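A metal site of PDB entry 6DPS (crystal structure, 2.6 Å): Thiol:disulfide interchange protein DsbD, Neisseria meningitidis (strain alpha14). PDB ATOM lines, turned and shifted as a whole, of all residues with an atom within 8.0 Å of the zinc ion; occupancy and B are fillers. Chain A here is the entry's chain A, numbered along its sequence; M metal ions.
A ring nitrogen (ND1) of His 74 lies within hydrogen-bond range of the side-chain carboxylate (OE2) of Glu 60, 2.6 Å away. The backbone carbonyl oxygen of Gly 33 is in hydrogen-bond range of the backbone NH of Glu 102, at 2.8 Å.
A ring nitrogen (NE2) of His 74 binds the zinc ion. The zinc ion is bound by OE2 of Glu 102 (2.2 Å). NZ of Lys 62 binds the zinc ion (2.2 Å). The zinc ion has three donor atoms within binding distance. Slightly farther from the zinc ion lies the side-chain carboxylate (OE1) of Glu 102 (2.8 Å).
Of the 15 residues printed, 3 come within 4 Å of the zinc ion.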
ATOM      1  N   GLY A  33       4.017 -30.812   4.448  1.00  0.00           N
ATOM      2  CA  GLY A  33       3.911 -30.808   5.899  1.00  0.00           C
ATOM      3  C   GLY A  33       5.012 -30.047   6.623  1.00  0.00           C
ATOM      4  O   GLY A  33       5.078 -30.124   7.865  1.00  0.00           O
ATOM      5  N   TYR A  34       5.874 -29.330   5.892  1.00  0.00           N
ATOM      6  CA  TYR A  34       6.953 -28.537   6.482  1.00  0.00           C
ATOM      7  C   TYR A  34       6.895 -27.136   5.902  1.00  0.00           C
ATOM      8  O   TYR A  34       6.201 -26.900   4.917  1.00  0.00           O
ATOM      9  CB  TYR A  34       8.323 -29.210   6.231  1.00  0.00           C
ATOM     10  CG  TYR A  34       8.390 -30.584   6.841  1.00  0.00           C
ATOM     11  CD1 TYR A  34       7.803 -31.674   6.208  1.00  0.00           C
ATOM     12  CD2 TYR A  34       9.002 -30.798   8.090  1.00  0.00           C
ATOM     13  CE1 TYR A  34       7.830 -32.927   6.782  1.00  0.00           C
ATOM     14  CE2 TYR A  34       9.032 -32.061   8.666  1.00  0.00           C
ATOM     15  CZ  TYR A  34       8.444 -33.133   7.999  1.00  0.00           C
ATOM     16  OH  TYR A  34       8.464 -34.403   8.534  1.00  0.00           O
ATOM     17  N   TYR A  35       7.598 -26.198   6.542  1.00  0.00           N
ATOM     18  CA  TYR A  35       7.681 -24.826   6.033  1.00  0.00           C
ATOM     19  C   TYR A  35       8.944 -24.172   6.541  1.00  0.00           C
ATOM     20  O   TYR A  35       9.623 -24.710   7.419  1.00  0.00           O
ATOM     21  CB  TYR A  35       6.483 -23.972   6.456  1.00  0.00           C
ATOM     22  CG  TYR A  35       6.328 -23.781   7.928  1.00  0.00           C
ATOM     23  CD1 TYR A  35       5.636 -24.712   8.700  1.00  0.00           C
ATOM     24  CD2 TYR A  35       6.819 -22.640   8.548  1.00  0.00           C
ATOM     25  CE1 TYR A  35       5.451 -24.522  10.054  1.00  0.00           C
ATOM     26  CE2 TYR A  35       6.642 -22.435   9.919  1.00  0.00           C
ATOM     27  CZ  TYR A  35       5.954 -23.390  10.657  1.00  0.00           C
ATOM     28  OH  TYR A  35       5.758 -23.225  12.004  1.00  0.00           O
ATOM     29  N   MET A  36       9.278 -23.010   5.970  1.00  0.00           N
ATOM     30  CA  MET A  36      10.559 -22.355   6.227  1.00  0.00           C
ATOM     31  C   MET A  36      10.367 -20.880   6.555  1.00  0.00           C
ATOM     32  O   MET A  36       9.493 -20.213   6.003  1.00  0.00           O
ATOM     33  CB  MET A  36      11.515 -22.474   5.024  1.00  0.00           C
ATOM     34  CG  MET A  36      12.118 -23.856   4.784  1.00  0.00           C
ATOM     35  SD  MET A  36      13.153 -23.819   3.305  1.00  0.00           S
ATOM     36  CE  MET A  36      14.696 -23.309   4.065  1.00  0.00           C
ATOM     37  N   GLU A  60       4.288 -16.623   2.082  1.00  0.00           N
ATOM     38  CA  GLU A  60       3.043 -16.347   2.780  1.00  0.00           C
ATOM     39  C   GLU A  60       3.279 -15.912   4.226  1.00  0.00           C
ATOM     40  O   GLU A  60       4.347 -16.130   4.809  1.00  0.00           O
ATOM     41  CB  GLU A  60       2.100 -17.549   2.800  1.00  0.00           C
ATOM     42  CG  GLU A  60       1.839 -18.109   1.446  1.00  0.00           C
ATOM     43  CD  GLU A  60       2.691 -19.305   1.191  1.00  0.00           C
ATOM     44  OE1 GLU A  60       3.403 -19.336   0.171  1.00  0.00           O
ATOM     45  OE2 GLU A  60       2.655 -20.200   2.040  1.00  0.00           O
ATOM     46  N   GLU A  61       2.241 -15.319   4.783  1.00  0.00           N
ATOM     47  CA  GLU A  61       2.267 -14.785   6.125  1.00  0.00           C
ATOM     48  C   GLU A  61       1.611 -15.804   7.046  1.00  0.00           C
ATOM     49  O   GLU A  61       0.637 -16.455   6.668  1.00  0.00           O
ATOM     50  CB  GLU A  61       1.530 -13.446   6.179  1.00  0.00           C
ATOM     51  CG  GLU A  61       1.524 -12.774   7.524  1.00  0.00           C
ATOM     52  CD  GLU A  61       0.966 -11.370   7.428  1.00  0.00           C
ATOM     53  OE1 GLU A  61      -0.158 -11.150   7.925  1.00  0.00           O
ATOM     54  OE2 GLU A  61       1.649 -10.506   6.850  1.00  0.00           O
ATOM     55  N   LYS A  62       2.194 -15.983   8.214  1.00  0.00           N
ATOM     56  CA  LYS A  62       1.676 -16.990   9.118  1.00  0.00           C
ATOM     57  C   LYS A  62       1.832 -16.500  10.537  1.00  0.00           C
ATOM     58  O   LYS A  62       2.863 -15.907  10.896  1.00  0.00           O
ATOM     59  CB  LYS A  62       2.385 -18.341   8.947  1.00  0.00           C
ATOM     60  CG  LYS A  62       2.261 -19.260  10.145  1.00  0.00           C
ATOM     61  CD  LYS A  62       3.132 -20.501   9.998  1.00  0.00           C
ATOM     62  CE  LYS A  62       2.686 -21.280   8.758  1.00  0.00           C
ATOM     63  NZ  LYS A  62       3.144 -22.690   8.711  1.00  0.00           N
ATOM     64  N   GLU A  63       0.816 -16.731  11.333  1.00  0.00           N
ATOM     65  CA  GLU A  63       0.907 -16.568  12.774  1.00  0.00           C
ATOM     66  C   GLU A  63       1.485 -17.861  13.343  1.00  0.00           C
ATOM     67  O   GLU A  63       0.869 -18.934  13.250  1.00  0.00           O
ATOM     68  CB  GLU A  63      -0.459 -16.236  13.389  1.00  0.00           C
ATOM     69  CG  GLU A  63      -0.543 -16.386  14.910  1.00  0.00           C
ATOM     70  CD  GLU A  63       0.588 -15.762  15.742  1.00  0.00           C
ATOM     71  OE1 GLU A  63       1.355 -14.873  15.234  1.00  0.00           O
ATOM     72  OE2 GLU A  63       0.662 -16.128  16.935  1.00  0.00           O
ATOM     73  N   ASP A  64       2.676 -17.780  13.864  1.00  0.00           N
ATOM     74  CA  ASP A  64       3.486 -18.910  14.248  1.00  0.00           C
ATOM     75  C   ASP A  64       3.627 -18.944  15.760  1.00  0.00           C
ATOM     76  O   ASP A  64       3.775 -17.923  16.429  1.00  0.00           O
ATOM     77  CB  ASP A  64       4.860 -18.825  13.542  1.00  0.00           C
ATOM     78  CG  ASP A  64       5.738 -19.972  13.859  1.00  0.00           C
ATOM     79  OD1 ASP A  64       6.491 -19.860  14.842  1.00  0.00           O
ATOM     80  OD2 ASP A  64       5.726 -20.968  13.104  1.00  0.00           O
ATOM     81  N   VAL A  72       6.617 -17.050   5.595  1.00  0.00           N
ATOM     82  CA  VAL A  72       7.095 -18.421   5.549  1.00  0.00           C
ATOM     83  C   VAL A  72       6.991 -18.957   4.132  1.00  0.00           C
ATOM     84  O   VAL A  72       6.460 -18.308   3.239  1.00  0.00           O
ATOM     85  CB  VAL A  72       6.358 -19.355   6.535  1.00  0.00           C
ATOM     86  CG1 VAL A  72       6.529 -18.851   7.940  1.00  0.00           C
ATOM     87  CG2 VAL A  72       4.889 -19.445   6.195  1.00  0.00           C
ATOM     88  N   TYR A  73       7.493 -20.166   3.952  1.00  0.00           N
ATOM     89  CA  TYR A  73       7.519 -20.826   2.652  1.00  0.00           C
ATOM     90  C   TYR A  73       7.000 -22.257   2.767  1.00  0.00           C
ATOM     91  O   TYR A  73       7.574 -23.080   3.490  1.00  0.00           O
ATOM     92  CB  TYR A  73       8.934 -20.842   2.073  1.00  0.00           C
ATOM     93  CG  TYR A  73       9.459 -19.510   1.603  1.00  0.00           C
ATOM     94  CD1 TYR A  73       8.921 -18.888   0.477  1.00  0.00           C
ATOM     95  CD2 TYR A  73      10.501 -18.880   2.264  1.00  0.00           C
ATOM     96  CE1 TYR A  73       9.408 -17.671   0.047  1.00  0.00           C
ATOM     97  CE2 TYR A  73      10.994 -17.682   1.836  1.00  0.00           C
ATOM     98  CZ  TYR A  73      10.450 -17.071   0.729  1.00  0.00           C
ATOM     99  OH  TYR A  73      10.944 -15.860   0.314  1.00  0.00           O
ATOM    100  N   HIS A  74       5.932 -22.552   2.047  1.00  0.00           N
ATOM    101  CA  HIS A  74       5.529 -23.915   1.752  1.00  0.00           C
ATOM    102  C   HIS A  74       5.983 -24.298   0.334  1.00  0.00           C
ATOM    103  O   HIS A  74       6.065 -23.455  -0.562  1.00  0.00           O
ATOM    104  CB  HIS A  74       4.016 -24.065   1.883  1.00  0.00           C
ATOM    105  CG  HIS A  74       3.465 -23.640   3.207  1.00  0.00           C
ATOM    106  ND1 HIS A  74       2.861 -22.421   3.413  1.00  0.00           N
ATOM    107  CD2 HIS A  74       3.451 -24.279   4.402  1.00  0.00           C
ATOM    108  CE1 HIS A  74       2.482 -22.325   4.681  1.00  0.00           C
ATOM    109  NE2 HIS A  74       2.832 -23.446   5.299  1.00  0.00           N
ATOM    110  N   CYS A 100      10.336 -25.809   9.873  1.00  0.00           N
ATOM    111  CA  CYS A 100       9.515 -26.438  10.903  1.00  0.00           C
ATOM    112  C   CYS A 100       8.585 -27.461  10.274  1.00  0.00           C
ATOM    113  O   CYS A 100       8.412 -27.502   9.046  1.00  0.00           O
ATOM    114  CB  CYS A 100       8.672 -25.395  11.685  1.00  0.00           C
ATOM    115  SG  CYS A 100       9.609 -24.046  12.464  1.00  0.00           S
ATOM    116  N   ALA A 101       7.950 -28.258  11.130  1.00  0.00           N
ATOM    117  CA  ALA A 101       6.892 -29.163  10.714  1.00  0.00           C
ATOM    118  C   ALA A 101       5.539 -28.575  11.104  1.00  0.00           C
ATOM    119  O   ALA A 101       5.394 -28.029  12.198  1.00  0.00           O
ATOM    120  CB  ALA A 101       7.094 -30.544  11.326  1.00  0.00           C
ATOM    121  N   GLU A 102       4.558 -28.700  10.214  1.00  0.00           N
ATOM    122  CA  GLU A 102       3.195 -28.234  10.489  1.00  0.00           C
ATOM    123  C   GLU A 102       2.578 -28.890  11.716  1.00  0.00           C
ATOM    124  O   GLU A 102       1.659 -28.316  12.312  1.00  0.00           O
ATOM    125  CB  GLU A 102       2.308 -28.511   9.276  1.00  0.00           C
ATOM    126  CG  GLU A 102       2.806 -27.835   8.011  1.00  0.00           C
ATOM    127  CD  GLU A 102       2.473 -26.354   7.936  1.00  0.00           C
ATOM    128  OE1 GLU A 102       1.951 -25.787   8.911  1.00  0.00           O
ATOM    129  OE2 GLU A 102       2.733 -25.767   6.878  1.00  0.00           O
HETATM  130 ZN    ZN M   1       2.041 -23.708   7.084  1.00  0.00          ZN
